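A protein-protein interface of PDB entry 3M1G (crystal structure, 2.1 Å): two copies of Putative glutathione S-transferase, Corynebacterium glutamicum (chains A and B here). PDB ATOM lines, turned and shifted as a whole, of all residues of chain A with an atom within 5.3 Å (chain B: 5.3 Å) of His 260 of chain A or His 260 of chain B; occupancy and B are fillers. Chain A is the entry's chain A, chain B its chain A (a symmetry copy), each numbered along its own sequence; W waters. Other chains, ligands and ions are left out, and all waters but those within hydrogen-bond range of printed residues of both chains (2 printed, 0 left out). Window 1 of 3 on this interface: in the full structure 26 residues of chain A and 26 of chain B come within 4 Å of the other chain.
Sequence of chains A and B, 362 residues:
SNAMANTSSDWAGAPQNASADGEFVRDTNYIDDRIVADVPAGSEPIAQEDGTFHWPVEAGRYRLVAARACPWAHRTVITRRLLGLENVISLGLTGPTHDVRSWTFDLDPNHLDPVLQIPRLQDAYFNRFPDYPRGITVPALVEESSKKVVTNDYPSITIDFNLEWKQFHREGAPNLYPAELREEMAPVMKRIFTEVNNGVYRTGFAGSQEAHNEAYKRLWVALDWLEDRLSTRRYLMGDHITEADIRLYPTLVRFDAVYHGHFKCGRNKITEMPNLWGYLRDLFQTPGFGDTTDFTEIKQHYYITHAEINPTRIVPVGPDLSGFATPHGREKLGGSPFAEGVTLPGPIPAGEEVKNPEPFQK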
ATOM      1  N   ARG A 254     -29.249   1.364  -3.195  1.00  0.00           N
ATOM      2  CA  ARG A 254     -29.379   2.726  -3.629  1.00  0.00           C
ATOM      3  C   ARG A 254     -28.013   3.377  -3.868  1.00  0.00           C
ATOM      4  O   ARG A 254     -27.929   4.547  -4.263  1.00  0.00           O
ATOM      5  CB  ARG A 254     -30.141   3.553  -2.576  1.00  0.00           C
ATOM      6  CG  ARG A 254     -31.617   3.222  -2.465  1.00  0.00           C
ATOM      7  CD  ARG A 254     -32.257   3.771  -1.189  1.00  0.00           C
ATOM      8  NE  ARG A 254     -33.695   3.532  -1.252  1.00  0.00           N
ATOM      9  CZ  ARG A 254     -34.268   2.335  -1.059  1.00  0.00           C
ATOM     10  NH1 ARG A 254     -33.533   1.298  -0.737  1.00  0.00           N
ATOM     11  NH2 ARG A 254     -35.585   2.187  -1.193  1.00  0.00           N
ATOM     12  N   PHE A 255     -26.949   2.652  -3.609  1.00  0.00           N
ATOM     13  CA  PHE A 255     -25.621   3.268  -3.619  1.00  0.00           C
ATOM     14  C   PHE A 255     -25.116   3.718  -4.993  1.00  0.00           C
ATOM     15  O   PHE A 255     -24.901   4.917  -5.218  1.00  0.00           O
ATOM     16  CB  PHE A 255     -24.588   2.387  -2.936  1.00  0.00           C
ATOM     17  CG  PHE A 255     -23.355   3.131  -2.544  1.00  0.00           C
ATOM     18  CD1 PHE A 255     -22.314   3.294  -3.447  1.00  0.00           C
ATOM     19  CD2 PHE A 255     -23.240   3.663  -1.301  1.00  0.00           C
ATOM     20  CE1 PHE A 255     -21.159   3.971  -3.092  1.00  0.00           C
ATOM     21  CE2 PHE A 255     -22.096   4.347  -0.916  1.00  0.00           C
ATOM     22  CZ  PHE A 255     -21.025   4.485  -1.841  1.00  0.00           C
ATOM     23  N   ASP A 256     -24.930   2.786  -5.912  1.00  0.00           N
ATOM     24  CA  ASP A 256     -24.448   3.178  -7.228  1.00  0.00           C
ATOM     25  C   ASP A 256     -25.461   4.076  -7.937  1.00  0.00           C
ATOM     26  O   ASP A 256     -25.070   5.049  -8.637  1.00  0.00           O
ATOM     27  CB  ASP A 256     -24.090   1.956  -8.092  1.00  0.00           C
ATOM     28  CG  ASP A 256     -22.841   1.214  -7.586  1.00  0.00           C
ATOM     29  OD1 ASP A 256     -22.167   1.744  -6.673  1.00  0.00           O
ATOM     30  OD2 ASP A 256     -22.550   0.096  -8.098  1.00  0.00           O
ATOM     31  N   VAL A 258     -27.654   6.303  -6.656  1.00  0.00           N
ATOM     32  CA  VAL A 258     -27.898   7.628  -6.069  1.00  0.00           C
ATOM     33  C   VAL A 258     -26.753   8.135  -5.195  1.00  0.00           C
ATOM     34  O   VAL A 258     -26.183   9.182  -5.452  1.00  0.00           O
ATOM     35  CB  VAL A 258     -29.187   7.669  -5.207  1.00  0.00           C
ATOM     36  CG1 VAL A 258     -29.257   9.014  -4.461  1.00  0.00           C
ATOM     37  CG2 VAL A 258     -30.430   7.462  -6.082  1.00  0.00           C
ATOM     38  N   TYR A 259     -26.400   7.402  -4.166  1.00  0.00           N
ATOM     39  CA  TYR A 259     -25.464   7.934  -3.164  1.00  0.00           C
ATOM     40  C   TYR A 259     -24.077   8.194  -3.728  1.00  0.00           C
ATOM     41  O   TYR A 259     -23.401   9.142  -3.338  1.00  0.00           O
ATOM     42  CB  TYR A 259     -25.339   6.985  -1.978  1.00  0.00           C
ATOM     43  CG  TYR A 259     -26.663   6.670  -1.239  1.00  0.00           C
ATOM     44  CD1 TYR A 259     -27.653   7.632  -1.065  1.00  0.00           C
ATOM     45  CD2 TYR A 259     -26.904   5.393  -0.726  1.00  0.00           C
ATOM     46  CE1 TYR A 259     -28.837   7.332  -0.370  1.00  0.00           C
ATOM     47  CE2 TYR A 259     -28.064   5.086  -0.053  1.00  0.00           C
ATOM     48  CZ  TYR A 259     -29.022   6.059   0.140  1.00  0.00           C
ATOM     49  OH  TYR A 259     -30.160   5.773   0.827  1.00  0.00           O
ATOM     50  N   HIS A 260     -23.642   7.335  -4.623  1.00  0.00           N
ATOM     51  CA  HIS A 260     -22.321   7.455  -5.280  1.00  0.00           C
ATOM     52  C   HIS A 260     -22.076   8.851  -5.849  1.00  0.00           C
ATOM     53  O   HIS A 260     -21.045   9.455  -5.563  1.00  0.00           O
ATOM     54  CB  HIS A 260     -22.180   6.368  -6.374  1.00  0.00           C
ATOM     55  CG  HIS A 260     -20.837   6.345  -7.042  1.00  0.00           C
ATOM     56  ND1 HIS A 260     -20.511   7.215  -8.067  1.00  0.00           N
ATOM     57  CD2 HIS A 260     -19.719   5.611  -6.793  1.00  0.00           C
ATOM     58  CE1 HIS A 260     -19.231   7.036  -8.400  1.00  0.00           C
ATOM     59  NE2 HIS A 260     -18.743   6.026  -7.681  1.00  0.00           N
ATOM     60  N   GLY A 261     -23.004   9.342  -6.676  1.00  0.00           N
ATOM     61  CA  GLY A 261     -22.904  10.666  -7.287  1.00  0.00           C
ATOM     62  C   GLY A 261     -23.640  11.792  -6.530  1.00  0.00           C
ATOM     63  O   GLY A 261     -23.022  12.756  -6.084  1.00  0.00           O
ATOM     64  N   HIS A 262     -24.957  11.649  -6.388  1.00  0.00           N
ATOM     65  CA  HIS A 262     -25.814  12.650  -5.741  1.00  0.00           C
ATOM     66  C   HIS A 262     -25.311  13.057  -4.355  1.00  0.00           C
ATOM     67  O   HIS A 262     -25.252  14.244  -4.064  1.00  0.00           O
ATOM     68  CB  HIS A 262     -27.244  12.103  -5.663  1.00  0.00           C
ATOM     69  CG  HIS A 262     -28.256  13.076  -5.139  1.00  0.00           C
ATOM     70  ND1 HIS A 262     -28.557  14.264  -5.776  1.00  0.00           N
ATOM     71  CD2 HIS A 262     -29.084  13.002  -4.059  1.00  0.00           C
ATOM     72  CE1 HIS A 262     -29.523  14.882  -5.109  1.00  0.00           C
ATOM     73  NE2 HIS A 262     -29.863  14.136  -4.063  1.00  0.00           N
ATOM     74  N   PHE A 263     -24.925  12.080  -3.532  1.00  0.00           N
ATOM     75  CA  PHE A 263     -24.376  12.336  -2.181  1.00  0.00           C
ATOM     76  C   PHE A 263     -22.840  12.336  -2.120  1.00  0.00           C
ATOM     77  O   PHE A 263     -22.255  12.380  -1.018  1.00  0.00           O
ATOM     78  CB  PHE A 263     -24.925  11.299  -1.177  1.00  0.00           C
ATOM     79  CG  PHE A 263     -26.373  11.519  -0.758  1.00  0.00           C
ATOM     80  CD1 PHE A 263     -27.087  12.633  -1.156  1.00  0.00           C
ATOM     81  CD2 PHE A 263     -26.965  10.660   0.133  1.00  0.00           C
ATOM     82  CE1 PHE A 263     -28.395  12.861  -0.697  1.00  0.00           C
ATOM     83  CE2 PHE A 263     -28.298  10.890   0.592  1.00  0.00           C
ATOM     84  CZ  PHE A 263     -28.999  11.979   0.146  1.00  0.00           C
ATOM     85  N   LYS A 264     -22.190  12.279  -3.287  1.00  0.00           N
ATOM     86  CA  LYS A 264     -20.723  12.380  -3.392  1.00  0.00           C
ATOM     87  C   LYS A 264     -19.998  11.327  -2.565  1.00  0.00           C
ATOM     88  O   LYS A 264     -18.889  11.556  -2.112  1.00  0.00           O
ATOM     89  CB  LYS A 264     -20.265  13.786  -2.995  1.00  0.00           C
ATOM     90  CG  LYS A 264     -20.921  14.927  -3.828  1.00  0.00           C
ATOM     91  CD  LYS A 264     -20.273  16.283  -3.543  1.00  0.00           C
ATOM     92  CE  LYS A 264     -20.768  17.384  -4.494  1.00  0.00           C
ATOM     93  NZ  LYS A 264     -22.196  17.780  -4.286  1.00  0.00           N
ATOM     94  N   CYS A 265     -20.600  10.141  -2.415  1.00  0.00           N
ATOM     95  CA  CYS A 265     -20.014   9.090  -1.583  1.00  0.00           C
ATOM     96  C   CYS A 265     -19.011   8.202  -2.360  1.00  0.00           C
ATOM     97  O   CYS A 265     -18.367   7.333  -1.781  1.00  0.00           O
ATOM     98  CB  CYS A 265     -21.105   8.174  -1.048  1.00  0.00           C
ATOM     99  SG  CYS A 265     -22.184   8.940   0.132  1.00  0.00           S
ATOM    100  N   GLY A 266     -18.907   8.423  -3.664  1.00  0.00           N
ATOM    101  CA  GLY A 266     -18.139   7.544  -4.559  1.00  0.00           C
ATOM    102  C   GLY A 266     -16.629   7.448  -4.506  1.00  0.00           C
ATOM    103  O   GLY A 266     -15.966   7.825  -5.474  1.00  0.00           O
ATOM    104  N   ARG A 267     -16.065   6.828  -3.453  1.00  0.00           N
ATOM    105  CA  ARG A 267     -14.664   6.392  -3.526  1.00  0.00           C
ATOM    106  C   ARG A 267     -14.538   5.340  -4.620  1.00  0.00           C
ATOM    107  O   ARG A 267     -13.566   5.318  -5.353  1.00  0.00           O
ATOM    108  CB  ARG A 267     -14.144   5.755  -2.245  1.00  0.00           C
ATOM    109  CG  ARG A 267     -12.628   5.484  -2.312  1.00  0.00           C
ATOM    110  CD  ARG A 267     -12.122   4.712  -1.104  1.00  0.00           C
ATOM    111  NE  ARG A 267     -12.545   3.309  -1.198  1.00  0.00           N
ATOM    112  CZ  ARG A 267     -12.383   2.404  -0.232  1.00  0.00           C
ATOM    113  NH1 ARG A 267     -11.862   2.748   0.936  1.00  0.00           N
ATOM    114  NH2 ARG A 267     -12.793   1.153  -0.421  1.00  0.00           N
ATOM    115  N   ASN A 268     -15.536   4.470  -4.670  1.00  0.00           N
ATOM    116  CA  ASN A 268     -15.618   3.337  -5.559  1.00  0.00           C
ATOM    117  C   ASN A 268     -17.088   3.070  -5.743  1.00  0.00           C
ATOM    118  O   ASN A 268     -17.892   3.488  -4.903  1.00  0.00           O
ATOM    119  CB  ASN A 268     -15.062   2.077  -4.896  1.00  0.00           C
ATOM    120  CG  ASN A 268     -13.578   2.065  -4.808  1.00  0.00           C
ATOM    121  OD1 ASN A 268     -13.014   2.136  -3.707  1.00  0.00           O
ATOM    122  ND2 ASN A 268     -12.915   1.877  -5.959  1.00  0.00           N
ATOM    123  N   LYS A 269     -17.443   2.367  -6.821  1.00  0.00           N
ATOM    124  CA  LYS A 269     -18.803   1.864  -6.966  1.00  0.00           C
ATOM    125  C   LYS A 269     -18.863   0.546  -6.158  1.00  0.00           C
ATOM    126  O   LYS A 269     -17.841  -0.120  -5.961  1.00  0.00           O
ATOM    127  CB  LYS A 269     -19.177   1.593  -8.435  1.00  0.00           C
ATOM    128  CG  LYS A 269     -19.531   2.852  -9.254  1.00  0.00           C
ATOM    129  CD  LYS A 269     -19.670   2.587 -10.756  1.00  0.00           C
ATOM    130  CE  LYS A 269     -20.940   1.757 -11.061  1.00  0.00           C
ATOM    131  NZ  LYS A 269     -21.243   1.642 -12.512  1.00  0.00           N
ATOM    132  N   ARG B 254     -10.308  12.922 -16.942  1.00  0.00           N
ATOM    133  CA  ARG B 254     -11.206  13.694 -16.131  1.00  0.00           C
ATOM    134  C   ARG B 254     -12.534  12.964 -15.905  1.00  0.00           C
ATOM    135  O   ARG B 254     -13.426  13.471 -15.214  1.00  0.00           O
ATOM    136  CB  ARG B 254     -11.497  15.052 -16.797  1.00  0.00           C
ATOM    137  CG  ARG B 254     -10.325  16.015 -16.796  1.00  0.00           C
ATOM    138  CD  ARG B 254     -10.511  17.181 -17.769  1.00  0.00           C
ATOM    139  NE  ARG B 254      -9.411  18.121 -17.582  1.00  0.00           N
ATOM    140  CZ  ARG B 254      -8.162  17.914 -18.023  1.00  0.00           C
ATOM    141  NH1 ARG B 254      -7.879  16.839 -18.718  1.00  0.00           N
ATOM    142  NH2 ARG B 254      -7.198  18.795 -17.759  1.00  0.00           N
ATOM    143  N   PHE B 255     -12.689  11.803 -16.498  1.00  0.00           N
ATOM    144  CA  PHE B 255     -13.998  11.146 -16.495  1.00  0.00           C
ATOM    145  C   PHE B 255     -14.475  10.638 -15.132  1.00  0.00           C
ATOM    146  O   PHE B 255     -15.495  11.111 -14.611  1.00  0.00           O
ATOM    147  CB  PHE B 255     -14.071  10.036 -17.530  1.00  0.00           C
ATOM    148  CG  PHE B 255     -15.471   9.639 -17.861  1.00  0.00           C
ATOM    149  CD1 PHE B 255     -16.132   8.687 -17.098  1.00  0.00           C
ATOM    150  CD2 PHE B 255     -16.118  10.209 -18.909  1.00  0.00           C
ATOM    151  CE1 PHE B 255     -17.427   8.301 -17.401  1.00  0.00           C
ATOM    152  CE2 PHE B 255     -17.415   9.844 -19.238  1.00  0.00           C
ATOM    153  CZ  PHE B 255     -18.072   8.848 -18.464  1.00  0.00           C
ATOM    154  N   ASP B 256     -13.758   9.696 -14.544  1.00  0.00           N
ATOM    155  CA  ASP B 256     -14.183   9.189 -13.249  1.00  0.00           C
ATOM    156  C   ASP B 256     -14.132  10.286 -12.187  1.00  0.00           C
ATOM    157  O   ASP B 256     -15.027  10.359 -11.301  1.00  0.00           O
ATOM    158  CB  ASP B 256     -13.362   7.961 -12.818  1.00  0.00           C
ATOM    159  CG  ASP B 256     -13.654   6.717 -13.675  1.00  0.00           C
ATOM    160  OD1 ASP B 256     -14.608   6.768 -14.485  1.00  0.00           O
ATOM    161  OD2 ASP B 256     -12.916   5.700 -13.541  1.00  0.00           O
ATOM    162  N   VAL B 258     -14.617  13.615 -12.485  1.00  0.00           N
ATOM    163  CA  VAL B 258     -15.552  14.739 -12.639  1.00  0.00           C
ATOM    164  C   VAL B 258     -16.781  14.405 -13.481  1.00  0.00           C
ATOM    165  O   VAL B 258     -17.905  14.510 -13.021  1.00  0.00           O
ATOM    166  CB  VAL B 258     -14.884  15.987 -13.272  1.00  0.00           C
ATOM    167  CG1 VAL B 258     -15.966  17.034 -13.596  1.00  0.00           C
ATOM    168  CG2 VAL B 258     -13.822  16.570 -12.330  1.00  0.00           C
ATOM    169  N   TYR B 259     -16.584  13.998 -14.713  1.00  0.00           N
ATOM    170  CA  TYR B 259     -17.717  13.874 -15.642  1.00  0.00           C
ATOM    171  C   TYR B 259     -18.716  12.810 -15.221  1.00  0.00           C
ATOM    172  O   TYR B 259     -19.920  12.956 -15.417  1.00  0.00           O
ATOM    173  CB  TYR B 259     -17.232  13.558 -17.052  1.00  0.00           C
ATOM    174  CG  TYR B 259     -16.254  14.591 -17.663  1.00  0.00           C
ATOM    175  CD1 TYR B 259     -16.385  15.955 -17.427  1.00  0.00           C
ATOM    176  CD2 TYR B 259     -15.197  14.173 -18.477  1.00  0.00           C
ATOM    177  CE1 TYR B 259     -15.501  16.878 -18.011  1.00  0.00           C
ATOM    178  CE2 TYR B 259     -14.320  15.069 -19.046  1.00  0.00           C
ATOM    179  CZ  TYR B 259     -14.482  16.420 -18.828  1.00  0.00           C
ATOM    180  OH  TYR B 259     -13.637  17.314 -19.407  1.00  0.00           O
ATOM    181  N   HIS B 260     -18.216  11.727 -14.668  1.00  0.00           N
ATOM    182  CA  HIS B 260     -19.055  10.605 -14.189  1.00  0.00           C
ATOM    183  C   HIS B 260     -20.197  11.073 -13.290  1.00  0.00           C
ATOM    184  O   HIS B 260     -21.348  10.719 -13.532  1.00  0.00           O
ATOM    185  CB  HIS B 260     -18.167   9.557 -13.473  1.00  0.00           C
ATOM    186  CG  HIS B 260     -18.908   8.333 -13.026  1.00  0.00           C
ATOM    187  ND1 HIS B 260     -19.640   8.304 -11.852  1.00  0.00           N
ATOM    188  CD2 HIS B 260     -19.089   7.122 -13.618  1.00  0.00           C
ATOM    189  CE1 HIS B 260     -20.268   7.131 -11.758  1.00  0.00           C
ATOM    190  NE2 HIS B 260     -19.903   6.371 -12.790  1.00  0.00           N
ATOM    191  N   GLY B 261     -19.873  11.836 -12.242  1.00  0.00           N
ATOM    192  CA  GLY B 261     -20.864  12.360 -11.304  1.00  0.00           C
ATOM    193  C   GLY B 261     -21.359  13.789 -11.608  1.00  0.00           C
ATOM    194  O   GLY B 261     -22.545  14.005 -11.846  1.00  0.00           O
ATOM    195  N   HIS B 262     -20.436  14.750 -11.606  1.00  0.00           N
ATOM    196  CA  HIS B 262     -20.744  16.169 -11.825  1.00  0.00           C
ATOM    197  C   HIS B 262     -21.560  16.411 -13.096  1.00  0.00           C
ATOM    198  O   HIS B 262     -22.542  17.139 -13.049  1.00  0.00           O
ATOM    199  CB  HIS B 262     -19.433  16.963 -11.859  1.00  0.00           C
ATOM    200  CG  HIS B 262     -19.606  18.449 -11.949  1.00  0.00           C
ATOM    201  ND1 HIS B 262     -20.236  19.193 -10.970  1.00  0.00           N
ATOM    202  CD2 HIS B 262     -19.171  19.339 -12.884  1.00  0.00           C
ATOM    203  CE1 HIS B 262     -20.186  20.476 -11.300  1.00  0.00           C
ATOM    204  NE2 HIS B 262     -19.543  20.593 -12.457  1.00  0.00           N
ATOM    205  N   PHE B 263     -21.170  15.777 -14.204  1.00  0.00           N
ATOM    206  CA  PHE B 263     -21.895  15.886 -15.490  1.00  0.00           C
ATOM    207  C   PHE B 263     -22.874  14.732 -15.755  1.00  0.00           C
ATOM    208  O   PHE B 263     -23.428  14.619 -16.869  1.00  0.00           O
ATOM    209  CB  PHE B 263     -20.892  15.982 -16.661  1.00  0.00           C
ATOM    210  CG  PHE B 263     -20.201  17.331 -16.802  1.00  0.00           C
ATOM    211  CD1 PHE B 263     -20.545  18.414 -16.015  1.00  0.00           C
ATOM    212  CD2 PHE B 263     -19.291  17.532 -17.810  1.00  0.00           C
ATOM    213  CE1 PHE B 263     -19.954  19.673 -16.212  1.00  0.00           C
ATOM    214  CE2 PHE B 263     -18.686  18.811 -18.002  1.00  0.00           C
ATOM    215  CZ  PHE B 263     -19.013  19.855 -17.178  1.00  0.00           C
ATOM    216  N   LYS B 264     -23.085  13.876 -14.750  1.00  0.00           N
ATOM    217  CA  LYS B 264     -24.076  12.787 -14.820  1.00  0.00           C
ATOM    218  C   LYS B 264     -23.843  11.851 -15.999  1.00  0.00           C
ATOM    219  O   LYS B 264     -24.780  11.266 -16.515  1.00  0.00           O
ATOM    220  CB  LYS B 264     -25.491  13.368 -14.865  1.00  0.00           C
ATOM    221  CG  LYS B 264     -25.835  14.300 -13.666  1.00  0.00           C
ATOM    222  CD  LYS B 264     -27.316  14.676 -13.644  1.00  0.00           C
ATOM    223  CE  LYS B 264     -27.715  15.429 -12.365  1.00  0.00           C
ATOM    224  NZ  LYS B 264     -27.142  16.807 -12.260  1.00  0.00           N
ATOM    225  N   CYS B 265     -22.578  11.661 -16.392  1.00  0.00           N
ATOM    226  CA  CYS B 265     -22.259  10.834 -17.557  1.00  0.00           C
ATOM    227  C   CYS B 265     -22.111   9.334 -17.202  1.00  0.00           C
ATOM    228  O   CYS B 265     -21.934   8.498 -18.083  1.00  0.00           O
ATOM    229  CB  CYS B 265     -20.942  11.282 -18.175  1.00  0.00           C
ATOM    230  SG  CYS B 265     -21.004  12.882 -18.935  1.00  0.00           S
ATOM    231  N   GLY B 266     -22.170   9.018 -15.914  1.00  0.00           N
ATOM    232  CA  GLY B 266     -21.865   7.669 -15.414  1.00  0.00           C
ATOM    233  C   GLY B 266     -22.754   6.477 -15.695  1.00  0.00           C
ATOM    234  O   GLY B 266     -23.330   5.920 -14.759  1.00  0.00           O
ATOM    235  N   ARG B 267     -22.780   5.980 -16.945  1.00  0.00           N
ATOM    236  CA  ARG B 267     -23.324   4.636 -17.187  1.00  0.00           C
ATOM    237  C   ARG B 267     -22.453   3.621 -16.459  1.00  0.00           C
ATOM    238  O   ARG B 267     -22.952   2.661 -15.899  1.00  0.00           O
ATOM    239  CB  ARG B 267     -23.339   4.228 -18.653  1.00  0.00           C
ATOM    240  CG  ARG B 267     -24.083   2.895 -18.870  1.00  0.00           C
ATOM    241  CD  ARG B 267     -23.977   2.397 -20.303  1.00  0.00           C
ATOM    242  NE  ARG B 267     -22.626   1.875 -20.549  1.00  0.00           N
ATOM    243  CZ  ARG B 267     -22.169   1.495 -21.742  1.00  0.00           C
ATOM    244  NH1 ARG B 267     -22.918   1.624 -22.826  1.00  0.00           N
ATOM    245  NH2 ARG B 267     -20.930   1.025 -21.858  1.00  0.00           N
ATOM    246  N   ASN B 268     -21.152   3.861 -16.520  1.00  0.00           N
ATOM    247  CA  ASN B 268     -20.115   3.014 -15.982  1.00  0.00           C
ATOM    248  C   ASN B 268     -18.958   3.928 -15.684  1.00  0.00           C
ATOM    249  O   ASN B 268     -18.881   5.020 -16.256  1.00  0.00           O
ATOM    250  CB  ASN B 268     -19.595   2.041 -17.040  1.00  0.00           C
ATOM    251  CG  ASN B 268     -20.537   0.927 -17.327  1.00  0.00           C
ATOM    252  OD1 ASN B 268     -21.096   0.847 -18.429  1.00  0.00           O
ATOM    253  ND2 ASN B 268     -20.658  -0.011 -16.375  1.00  0.00           N
ATOM    254  N   LYS B 269     -18.051   3.487 -14.808  1.00  0.00           N
ATOM    255  CA  LYS B 269     -16.788   4.191 -14.627  1.00  0.00           C
ATOM    256  C   LYS B 269     -15.854   3.694 -15.756  1.00  0.00           C
ATOM    257  O   LYS B 269     -16.018   2.582 -16.268  1.00  0.00           O
ATOM    258  CB  LYS B 269     -16.146   3.906 -13.256  1.00  0.00           C
ATOM    259  CG  LYS B 269     -16.772   4.680 -12.078  1.00  0.00           C
ATOM    260  CD  LYS B 269     -16.280   4.212 -10.705  1.00  0.00           C
ATOM    261  CE  LYS B 269     -14.802   4.611 -10.476  1.00  0.00           C
ATOM    262  NZ  LYS B 269     -14.326   4.369  -9.088  1.00  0.00           N
HETATM  263  O   HOH W   1     -21.616   4.278 -13.079  1.00  0.00           O
HETATM  264  O   HOH W   2     -16.024   6.032  -7.761  1.00  0.00           O
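The backbone NH (N) of Cys 265 of chain A is in hydrogen-bond range of the backbone carbonyl oxygen (O) of His 260 of chain A (3.3 Å).
The guanidinium group (NE) of Arg 267 of chain A lies within hydrogen-bond range of the side-chain amide oxygen (OD1) of Asn 268 of chain A (2.8 Å).
O of Phe 255 of chain B sits at hydrogen-bond distance from N of His 260 of chain B (2.8 Å).
The backbone carbonyl oxygen (O) of His 260 of chain B lies within hydrogen-bond range of the backbone NH (N) of Cys 265 of chain B, at 3.3 Å.
The backbone NH of Gly 266 of chain B is in hydrogen-bond range of the backbone carbonyl oxygen of His 260 of chain B (3.0 Å).
The side-chain amide oxygen of Asn 268 of chain B is in hydrogen-bond range of the guanidinium group of Arg 267 of chain B (2.8 Å).
Among the printed residues, merely in contact across the chains: His 260 of chain A with His 260 of chain B (3.5 Å), Lys 269 of chain A with Lys 269 of chain B (3.8 Å), Asn 268 of chain A with Lys 269 of chain B (3.9 Å), Lys 269 of chain A with Asn 268 of chain B (3.9 Å), Arg 267 of chain A with Lys 269 of chain B (3.9 Å) and Lys 269 of chain A with Arg 267 of chain B (3.9 Å).
His 260 of chain A touches just one residue of chain B: His 260.
Of the printed residues of chain A, His 260 of chain B touches His 260.
Of the printed residues of chain B, Asn 268 of chain A touches Lys 269 (3.9 Å).
Of the printed residues of chain A, Asn 268 of chain B touches Lys 269 (3.9 Å).
Printed residues of chain B within 4 Å of Arg 267 of chain A: Lys 269 (3.9 Å).
The nearest residue of chain B that does not touch His 260 of chain A is Lys 269 of chain B (4.3 Å).
The nearest printed residue of chain A that does not touch Arg 267 of chain B is Asp 256 of chain A (7.9 Å).
Among the printed residues, no Asp or Glu carboxylate lies within 4 Å of a Lys or Arg side-chain nitrogen of the other chain.
His 260 of chain A touches its own counterpart, His 260 of chain B.
Arg 267 of chain A touches Lys 269 of chain B, and with the chains exchanged Lys 269 of chain A touches Arg 267 of chain B.
Asn 268 of chain A touches Lys 269 of chain B, and with the chains exchanged Lys 269 of chain A touches Asn 268 of chain B.
Lys 269 of chain A touches its own counterpart, Lys 269 of chain B.
Positions printed for both chains: 254, 255, 256, 258, 259, 260, 261, 262, 263, 264, 265, 266, 267, 268 and 269.
Of the 6 pairs that touch across the chains among the printed residues, 6 have their exchanged pair printed and touching as well.
Water W2 lies within hydrogen-bond range of NE2 of His 260 of chain A (2.7 Å), NZ of Lys 269 of chain B (2.7 Å), O of Gly 266 of chain A (2.9 Å) and N of Asn 268 of chain A (3.5 Å).
Water W1 lies within hydrogen-bond range of NE2 of His 260 of chain B (2.7 Å), NZ of Lys 269 of chain A (2.7 Å), O of Gly 266 of chain B (2.9 Å) and N of Asn 268 of chain B (3.5 Å).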
